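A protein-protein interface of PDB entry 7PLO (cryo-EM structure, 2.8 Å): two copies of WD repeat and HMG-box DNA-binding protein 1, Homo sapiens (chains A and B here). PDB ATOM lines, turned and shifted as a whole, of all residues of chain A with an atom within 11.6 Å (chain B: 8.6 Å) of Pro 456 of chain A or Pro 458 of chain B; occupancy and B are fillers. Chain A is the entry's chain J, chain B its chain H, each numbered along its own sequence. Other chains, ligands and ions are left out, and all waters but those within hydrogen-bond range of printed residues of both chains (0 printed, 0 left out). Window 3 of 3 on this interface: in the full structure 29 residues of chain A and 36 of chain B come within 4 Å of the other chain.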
ATOM      1  N   GLY A 455      20.855  22.810 -16.745  1.00  0.00           N
ATOM      2  CA  GLY A 455      21.037  22.455 -15.350  1.00  0.00           C
ATOM      3  C   GLY A 455      19.778  22.661 -14.524  1.00  0.00           C
ATOM      4  O   GLY A 455      18.754  23.083 -15.061  1.00  0.00           O
ATOM      5  N   PRO A 456      19.840  22.365 -13.224  1.00  0.00           N
ATOM      6  CA  PRO A 456      18.659  22.555 -12.372  1.00  0.00           C
ATOM      7  C   PRO A 456      18.259  24.019 -12.254  1.00  0.00           C
ATOM      8  O   PRO A 456      19.069  24.934 -12.428  1.00  0.00           O
ATOM      9  CB  PRO A 456      19.100  21.991 -11.016  1.00  0.00           C
ATOM     10  CG  PRO A 456      20.211  21.063 -11.330  1.00  0.00           C
ATOM     11  CD  PRO A 456      20.922  21.669 -12.499  1.00  0.00           C
ATOM     12  N   MET A 457      16.978  24.223 -11.948  1.00  0.00           N
ATOM     13  CA  MET A 457      16.339  25.524 -11.828  1.00  0.00           C
ATOM     14  C   MET A 457      15.860  25.722 -10.391  1.00  0.00           C
ATOM     15  O   MET A 457      15.128  24.862  -9.880  1.00  0.00           O
ATOM     16  CB  MET A 457      15.142  25.612 -12.804  1.00  0.00           C
ATOM     17  CG  MET A 457      14.305  26.896 -12.737  1.00  0.00           C
ATOM     18  SD  MET A 457      15.231  28.406 -13.078  1.00  0.00           S
ATOM     19  CE  MET A 457      15.551  28.235 -14.832  1.00  0.00           C
ATOM     20  N   PRO A 458      16.229  26.810  -9.697  1.00  0.00           N
ATOM     21  CA  PRO A 458      15.675  27.020  -8.352  1.00  0.00           C
ATOM     22  C   PRO A 458      14.178  27.281  -8.382  1.00  0.00           C
ATOM     23  O   PRO A 458      13.629  27.800  -9.359  1.00  0.00           O
ATOM     24  CB  PRO A 458      16.442  28.241  -7.831  1.00  0.00           C
ATOM     25  CG  PRO A 458      16.932  28.928  -9.037  1.00  0.00           C
ATOM     26  CD  PRO A 458      17.243  27.839 -10.004  1.00  0.00           C
ATOM     27  N   THR A 459      13.515  26.916  -7.278  1.00  0.00           N
ATOM     28  CA  THR A 459      12.070  26.986  -7.124  1.00  0.00           C
ATOM     29  C   THR A 459      11.661  28.227  -6.341  1.00  0.00           C
ATOM     30  O   THR A 459      12.479  28.824  -5.635  1.00  0.00           O
ATOM     31  CB  THR A 459      11.543  25.751  -6.385  1.00  0.00           C
ATOM     32  OG1 THR A 459      12.191  25.634  -5.112  1.00  0.00           O
ATOM     33  CG2 THR A 459      11.780  24.497  -7.190  1.00  0.00           C
ATOM     34  N   PRO A 460      10.397  28.646  -6.430  1.00  0.00           N
ATOM     35  CA  PRO A 460       9.873  29.589  -5.437  1.00  0.00           C
ATOM     36  C   PRO A 460       9.639  28.894  -4.104  1.00  0.00           C
ATOM     37  O   PRO A 460       9.535  27.668  -4.018  1.00  0.00           O
ATOM     38  CB  PRO A 460       8.559  30.074  -6.057  1.00  0.00           C
ATOM     39  CG  PRO A 460       8.135  28.963  -6.935  1.00  0.00           C
ATOM     40  CD  PRO A 460       9.398  28.370  -7.482  1.00  0.00           C
ATOM     41  N   THR A 623      17.202  26.561  -0.362  1.00  0.00           N
ATOM     42  CA  THR A 623      16.444  26.612  -1.607  1.00  0.00           C
ATOM     43  C   THR A 623      16.448  25.235  -2.258  1.00  0.00           C
ATOM     44  O   THR A 623      17.459  24.526  -2.221  1.00  0.00           O
ATOM     45  CB  THR A 623      17.035  27.658  -2.574  1.00  0.00           C
ATOM     46  OG1 THR A 623      17.041  28.945  -1.945  1.00  0.00           O
ATOM     47  CG2 THR A 623      16.228  27.741  -3.874  1.00  0.00           C
ATOM     48  N   GLY A 624      15.307  24.872  -2.858  1.00  0.00           N
ATOM     49  CA  GLY A 624      15.169  23.636  -3.596  1.00  0.00           C
ATOM     50  C   GLY A 624      15.180  23.876  -5.096  1.00  0.00           C
ATOM     51  O   GLY A 624      14.953  24.990  -5.564  1.00  0.00           O
ATOM     52  N   PHE A 625      15.445  22.803  -5.847  1.00  0.00           N
ATOM     53  CA  PHE A 625      15.665  22.869  -7.287  1.00  0.00           C
ATOM     54  C   PHE A 625      14.870  21.779  -7.989  1.00  0.00           C
ATOM     55  O   PHE A 625      14.789  20.645  -7.504  1.00  0.00           O
ATOM     56  CB  PHE A 625      17.160  22.725  -7.623  1.00  0.00           C
ATOM     57  CG  PHE A 625      18.026  23.801  -7.023  1.00  0.00           C
ATOM     58  CD1 PHE A 625      18.464  23.708  -5.710  1.00  0.00           C
ATOM     59  CD2 PHE A 625      18.410  24.899  -7.773  1.00  0.00           C
ATOM     60  CE1 PHE A 625      19.252  24.695  -5.155  1.00  0.00           C
ATOM     61  CE2 PHE A 625      19.205  25.887  -7.223  1.00  0.00           C
ATOM     62  CZ  PHE A 625      19.628  25.784  -5.913  1.00  0.00           C
ATOM     63  N   ASP A 626      14.295  22.130  -9.143  1.00  0.00           N
ATOM     64  CA  ASP A 626      13.515  21.204  -9.970  1.00  0.00           C
ATOM     65  C   ASP A 626      12.347  20.607  -9.186  1.00  0.00           C
ATOM     66  O   ASP A 626      12.163  19.390  -9.122  1.00  0.00           O
ATOM     67  CB  ASP A 626      14.407  20.102 -10.548  1.00  0.00           C
ATOM     68  CG  ASP A 626      15.537  20.652 -11.398  1.00  0.00           C
ATOM     69  OD1 ASP A 626      15.413  21.794 -11.890  1.00  0.00           O
ATOM     70  OD2 ASP A 626      16.547  19.940 -11.579  1.00  0.00           O
ATOM     71  N   GLY A 627      11.549  21.487  -8.583  1.00  0.00           N
ATOM     72  CA  GLY A 627      10.385  21.096  -7.819  1.00  0.00           C
ATOM     73  C   GLY A 627      10.645  20.757  -6.366  1.00  0.00           C
ATOM     74  O   GLY A 627       9.683  20.622  -5.599  1.00  0.00           O
ATOM     75  N   ASP A 628      11.905  20.619  -5.958  1.00  0.00           N
ATOM     76  CA  ASP A 628      12.213  20.264  -4.582  1.00  0.00           C
ATOM     77  C   ASP A 628      12.003  21.464  -3.661  1.00  0.00           C
ATOM     78  O   ASP A 628      11.989  22.620  -4.094  1.00  0.00           O
ATOM     79  CB  ASP A 628      13.655  19.755  -4.480  1.00  0.00           C
ATOM     80  CG  ASP A 628      13.940  19.035  -3.171  1.00  0.00           C
ATOM     81  OD1 ASP A 628      13.022  18.918  -2.332  1.00  0.00           O
ATOM     82  OD2 ASP A 628      15.090  18.586  -2.981  1.00  0.00           O
ATOM     83  N   GLN A 629      11.819  21.170  -2.372  1.00  0.00           N
ATOM     84  CA  GLN A 629      11.686  22.173  -1.323  1.00  0.00           C
ATOM     85  C   GLN A 629      12.628  21.826  -0.179  1.00  0.00           C
ATOM     86  O   GLN A 629      12.819  20.649   0.143  1.00  0.00           O
ATOM     87  CB  GLN A 629      10.239  22.264  -0.816  1.00  0.00           C
ATOM     88  CG  GLN A 629       9.257  22.832  -1.835  1.00  0.00           C
ATOM     89  CD  GLN A 629       9.459  24.317  -2.080  1.00  0.00           C
ATOM     90  OE1 GLN A 629       8.901  25.155  -1.372  1.00  0.00           O
ATOM     91  NE2 GLN A 629      10.259  24.649  -3.087  1.00  0.00           N
ATOM     92  N   ARG A 655       9.726  13.255  -2.072  1.00  0.00           N
ATOM     93  CA  ARG A 655      10.357  13.961  -3.181  1.00  0.00           C
ATOM     94  C   ARG A 655       9.357  14.853  -3.907  1.00  0.00           C
ATOM     95  O   ARG A 655       8.274  14.406  -4.297  1.00  0.00           O
ATOM     96  CB  ARG A 655      10.973  12.950  -4.150  1.00  0.00           C
ATOM     97  CG  ARG A 655      11.752  13.562  -5.305  1.00  0.00           C
ATOM     98  CD  ARG A 655      12.543  12.499  -6.058  1.00  0.00           C
ATOM     99  NE  ARG A 655      13.259  13.065  -7.203  1.00  0.00           N
ATOM    100  CZ  ARG A 655      13.187  12.665  -8.471  1.00  0.00           C
ATOM    101  NH1 ARG A 655      12.461  11.620  -8.847  1.00  0.00           N
ATOM    102  NH2 ARG A 655      13.877  13.328  -9.395  1.00  0.00           N
ATOM    103  N   LYS A 656       9.732  16.123  -4.084  1.00  0.00           N
ATOM    104  CA  LYS A 656       8.915  17.122  -4.780  1.00  0.00           C
ATOM    105  C   LYS A 656       7.548  17.311  -4.122  1.00  0.00           C
ATOM    106  O   LYS A 656       6.568  17.657  -4.788  1.00  0.00           O
ATOM    107  CB  LYS A 656       8.751  16.765  -6.262  1.00  0.00           C
ATOM    108  CG  LYS A 656      10.051  16.797  -7.056  1.00  0.00           C
ATOM    109  CD  LYS A 656       9.897  16.164  -8.437  1.00  0.00           C
ATOM    110  CE  LYS A 656       8.975  16.967  -9.351  1.00  0.00           C
ATOM    111  NZ  LYS A 656       8.870  16.353 -10.702  1.00  0.00           N
ATOM    112  N   GLY B 455      23.456  34.776 -14.209  1.00  0.00           N
ATOM    113  CA  GLY B 455      23.661  34.666 -12.776  1.00  0.00           C
ATOM    114  C   GLY B 455      24.452  33.428 -12.391  1.00  0.00           C
ATOM    115  O   GLY B 455      24.954  32.721 -13.266  1.00  0.00           O
ATOM    116  N   PRO B 456      24.580  33.170 -11.087  1.00  0.00           N
ATOM    117  CA  PRO B 456      25.277  31.957 -10.642  1.00  0.00           C
ATOM    118  C   PRO B 456      24.588  30.691 -11.133  1.00  0.00           C
ATOM    119  O   PRO B 456      23.364  30.633 -11.265  1.00  0.00           O
ATOM    120  CB  PRO B 456      25.235  32.062  -9.113  1.00  0.00           C
ATOM    121  CG  PRO B 456      25.089  33.516  -8.839  1.00  0.00           C
ATOM    122  CD  PRO B 456      24.251  34.059  -9.957  1.00  0.00           C
ATOM    123  N   MET B 457      25.405  29.666 -11.398  1.00  0.00           N
ATOM    124  CA  MET B 457      24.948  28.428 -12.021  1.00  0.00           C
ATOM    125  C   MET B 457      24.827  27.332 -10.972  1.00  0.00           C
ATOM    126  O   MET B 457      25.858  26.959 -10.388  1.00  0.00           O
ATOM    127  CB  MET B 457      25.926  28.003 -13.110  1.00  0.00           C
ATOM    128  CG  MET B 457      25.537  26.725 -13.846  1.00  0.00           C
ATOM    129  SD  MET B 457      26.296  25.228 -13.176  1.00  0.00           S
ATOM    130  CE  MET B 457      27.988  25.411 -13.737  1.00  0.00           C
ATOM    131  N   PRO B 458      23.643  26.777 -10.683  1.00  0.00           N
ATOM    132  CA  PRO B 458      23.594  25.592  -9.816  1.00  0.00           C
ATOM    133  C   PRO B 458      24.018  24.339 -10.568  1.00  0.00           C
ATOM    134  O   PRO B 458      23.681  24.150 -11.740  1.00  0.00           O
ATOM    135  CB  PRO B 458      22.120  25.510  -9.391  1.00  0.00           C
ATOM    136  CG  PRO B 458      21.471  26.762  -9.880  1.00  0.00           C
ATOM    137  CD  PRO B 458      22.284  27.231 -11.028  1.00  0.00           C
ATOM    138  N   THR B 459      24.757  23.474  -9.875  1.00  0.00           N
ATOM    139  CA  THR B 459      25.278  22.259 -10.480  1.00  0.00           C
ATOM    140  C   THR B 459      24.241  21.136 -10.442  1.00  0.00           C
ATOM    141  O   THR B 459      23.288  21.188  -9.659  1.00  0.00           O
ATOM    142  CB  THR B 459      26.537  21.803  -9.751  1.00  0.00           C
ATOM    143  OG1 THR B 459      26.274  21.716  -8.345  1.00  0.00           O
ATOM    144  CG2 THR B 459      27.672  22.771  -9.994  1.00  0.00           C
ATOM    145  N   PRO B 460      24.397  20.105 -11.275  1.00  0.00           N
ATOM    146  CA  PRO B 460      23.576  18.902 -11.108  1.00  0.00           C
ATOM    147  C   PRO B 460      24.069  18.045  -9.953  1.00  0.00           C
ATOM    148  O   PRO B 460      25.251  18.043  -9.604  1.00  0.00           O
ATOM    149  CB  PRO B 460      23.743  18.172 -12.445  1.00  0.00           C
ATOM    150  CG  PRO B 460      25.086  18.571 -12.909  1.00  0.00           C
ATOM    151  CD  PRO B 460      25.260  19.997 -12.470  1.00  0.00           C
ATOM    152  N   ARG B 461      23.135  17.308  -9.358  1.00  0.00           N
ATOM    153  CA  ARG B 461      23.483  16.389  -8.284  1.00  0.00           C
ATOM    154  C   ARG B 461      24.208  15.172  -8.852  1.00  0.00           C
ATOM    155  O   ARG B 461      23.779  14.594  -9.855  1.00  0.00           O
ATOM    156  CB  ARG B 461      22.227  15.958  -7.529  1.00  0.00           C
ATOM    157  CG  ARG B 461      21.609  17.060  -6.679  1.00  0.00           C
ATOM    158  CD  ARG B 461      20.268  16.636  -6.101  1.00  0.00           C
ATOM    159  NE  ARG B 461      19.737  17.619  -5.163  1.00  0.00           N
ATOM    160  CZ  ARG B 461      18.515  17.597  -4.641  1.00  0.00           C
ATOM    161  NH1 ARG B 461      17.637  16.656  -4.958  1.00  0.00           N
ATOM    162  NH2 ARG B 461      18.162  18.546  -3.780  1.00  0.00           N
ATOM    163  N   GLY B 622      21.587  19.864  -0.668  1.00  0.00           N
ATOM    164  CA  GLY B 622      21.072  20.820  -1.627  1.00  0.00           C
ATOM    165  C   GLY B 622      21.725  20.568  -2.969  1.00  0.00           C
ATOM    166  O   GLY B 622      21.775  19.423  -3.428  1.00  0.00           O
ATOM    167  N   THR B 623      22.215  21.623  -3.617  1.00  0.00           N
ATOM    168  CA  THR B 623      23.130  21.473  -4.738  1.00  0.00           C
ATOM    169  C   THR B 623      24.165  22.586  -4.673  1.00  0.00           C
ATOM    170  O   THR B 623      23.902  23.668  -4.141  1.00  0.00           O
ATOM    171  CB  THR B 623      22.404  21.485  -6.098  1.00  0.00           C
ATOM    172  OG1 THR B 623      23.258  20.922  -7.100  1.00  0.00           O
ATOM    173  CG2 THR B 623      22.010  22.900  -6.519  1.00  0.00           C
ATOM    174  N   GLY B 624      25.347  22.307  -5.222  1.00  0.00           N
ATOM    175  CA  GLY B 624      26.425  23.270  -5.241  1.00  0.00           C
ATOM    176  C   GLY B 624      26.324  24.223  -6.419  1.00  0.00           C
ATOM    177  O   GLY B 624      25.379  24.190  -7.206  1.00  0.00           O
ATOM    178  N   PHE B 625      27.332  25.090  -6.524  1.00  0.00           N
ATOM    179  CA  PHE B 625      27.378  26.137  -7.537  1.00  0.00           C
ATOM    180  C   PHE B 625      28.773  26.213  -8.139  1.00  0.00           C
ATOM    181  O   PHE B 625      29.767  26.230  -7.407  1.00  0.00           O
ATOM    182  CB  PHE B 625      26.994  27.497  -6.940  1.00  0.00           C
ATOM    183  CG  PHE B 625      25.511  27.734  -6.865  1.00  0.00           C
ATOM    184  CD1 PHE B 625      24.742  27.114  -5.895  1.00  0.00           C
ATOM    185  CD2 PHE B 625      24.889  28.588  -7.761  1.00  0.00           C
ATOM    186  CE1 PHE B 625      23.379  27.333  -5.825  1.00  0.00           C
ATOM    187  CE2 PHE B 625      23.528  28.812  -7.695  1.00  0.00           C
ATOM    188  CZ  PHE B 625      22.772  28.185  -6.725  1.00  0.00           C
ATOM    189  N   ASP B 626      28.832  26.266  -9.471  1.00  0.00           N
ATOM    190  CA  ASP B 626      30.075  26.456 -10.221  1.00  0.00           C
ATOM    191  C   ASP B 626      31.087  25.349  -9.915  1.00  0.00           C
ATOM    192  O   ASP B 626      32.176  25.586  -9.386  1.00  0.00           O
ATOM    193  CB  ASP B 626      30.668  27.842  -9.941  1.00  0.00           C
ATOM    194  CG  ASP B 626      31.768  28.222 -10.922  1.00  0.00           C
ATOM    195  OD1 ASP B 626      32.028  27.450 -11.870  1.00  0.00           O
ATOM    196  OD2 ASP B 626      32.373  29.300 -10.745  1.00  0.00           O
ATOM    197  N   GLY B 627      30.701  24.121 -10.261  1.00  0.00           N
ATOM    198  CA  GLY B 627      31.563  22.965 -10.154  1.00  0.00           C
ATOM    199  C   GLY B 627      31.466  22.195  -8.852  1.00  0.00           C
ATOM    200  O   GLY B 627      31.864  21.025  -8.814  1.00  0.00           O
ATOM    201  N   ASP B 628      30.943  22.806  -7.792  1.00  0.00           N
ATOM    202  CA  ASP B 628      30.845  22.171  -6.487  1.00  0.00           C
ATOM    203  C   ASP B 628      29.502  21.457  -6.347  1.00  0.00           C
ATOM    204  O   ASP B 628      28.573  21.674  -7.130  1.00  0.00           O
ATOM    205  CB  ASP B 628      31.015  23.219  -5.379  1.00  0.00           C
ATOM    206  CG  ASP B 628      31.371  22.609  -4.028  1.00  0.00           C
ATOM    207  OD1 ASP B 628      31.460  21.368  -3.921  1.00  0.00           O
ATOM    208  OD2 ASP B 628      31.557  23.382  -3.064  1.00  0.00           O
ATOM    209  N   GLN B 629      29.416  20.583  -5.343  1.00  0.00           N
ATOM    210  CA  GLN B 629      28.175  19.911  -4.981  1.00  0.00           C
ATOM    211  C   GLN B 629      28.029  19.913  -3.466  1.00  0.00           C
ATOM    212  O   GLN B 629      29.021  19.951  -2.732  1.00  0.00           O
ATOM    213  CB  GLN B 629      28.119  18.466  -5.511  1.00  0.00           C
ATOM    214  CG  GLN B 629      27.599  18.322  -6.954  1.00  0.00           C
ATOM    215  CD  GLN B 629      28.692  18.270  -8.016  1.00  0.00           C
ATOM    216  OE1 GLN B 629      29.883  18.393  -7.726  1.00  0.00           O
ATOM    217  NE2 GLN B 629      28.278  18.084  -9.266  1.00  0.00           N
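Printed residues of chain B within 4 Å of Pro 456 of chain A: Pro 458 (3.8 Å) and Thr 459 (3.5 Å). Pro 458 of chain B touches two residues of chain A. Gly 455 of chain A touches none of the printed residues of chain B. No residue of chain A comes within 4 Å of Met 457 of chain B. Of chain A, only Pro 456 (3.5 Å) comes within 4 Å of Thr 459 of chain B. Thr 623 of chain B touches one residue of chain A. No residue of chain A comes within 4 Å of Gly 624 of chain B. Of the printed residues of chain B, Asp 628 of chain A touches Arg 461. Of the printed residues of chain B, Phe 625 of chain A touches Pro 458 and Thr 623. Of the printed residues of chain A, Arg 461 of chain B touches Asp 628 (3.2 Å). Gly 627 of chain B touches none of the printed residues of chain A. Pro 460 of chain A touches none of the printed residues of chain B. The nearest printed residue of chain A that does not touch Arg 461 of chain B is Pro 456 of chain A (5.2 Å).
Pro 456 of chain A touches Pro 458 of chain B. Thr 459 of chain B touches Pro 456 of chain A (O to CG, 3.5 Å). CG of Pro 458 of chain B touches CE2 of Phe 625 of chain A, 3.6 Å away. Phe 625 of chain A touches Thr 623 of chain B (CE1 to CG2, 3.6 Å).
Of the 15 printed residues of chain B, 4 touch a printed residue of chain A. Among the printed residues, Asp or Glu carboxylates within 4 Å of a Lys or Arg side-chain nitrogen of the other chain: Asp 628 of chain A with Arg 461 of chain B (3.2 Å).
The backbone carbonyl oxygen of Thr 459 of chain B sits at hydrogen-bond distance from the side-chain hydroxyl of Thr 623 of chain B, at 2.6 Å. The backbone carbonyl oxygen (O) of Gly 624 of chain B sits at hydrogen-bond distance from the backbone NH (N) of Thr 459 of chain B (2.8 Å). The backbone carbonyl oxygen of Asp 628 of chain B sits at hydrogen-bond distance from the side-chain hydroxyl of Thr 459 of chain B. The guanidinium group of Arg 461 of chain B lies within hydrogen-bond range of the backbone carbonyl oxygen of Gly 622 of chain B (3.2 Å). O of Asp 628 of chain A lies within hydrogen-bond range of OG1 of Thr 459 of chain A, at 3.2 Å.
Pro 456 of chain A touches Pro 458 of chain B, but with the chains exchanged Pro 458 of chain A does not touch Pro 456 of chain B (6.8 Å). Pro 456 of chain A touches Thr 459 of chain B, but with the chains exchanged Thr 459 of chain A does not touch Pro 456 of chain B (11.3 Å). Phe 625 of chain A touches Pro 458 of chain B, but with the chains exchanged Pro 458 of chain A does not touch Phe 625 of chain B (6.3 Å). Phe 625 of chain A touches Thr 623 of chain B, but with the chains exchanged Thr 623 of chain A does not touch Phe 625 of chain B (7.1 Å). Of the 5 pairs that touch across the chains among the printed residues, none has its exchanged pair printed and touching as well.
The guanidinium group (NH2) of Arg 461 of chain B is in salt-bridge range of the side-chain carboxylate (OD2) of Asp 628 of chain A.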
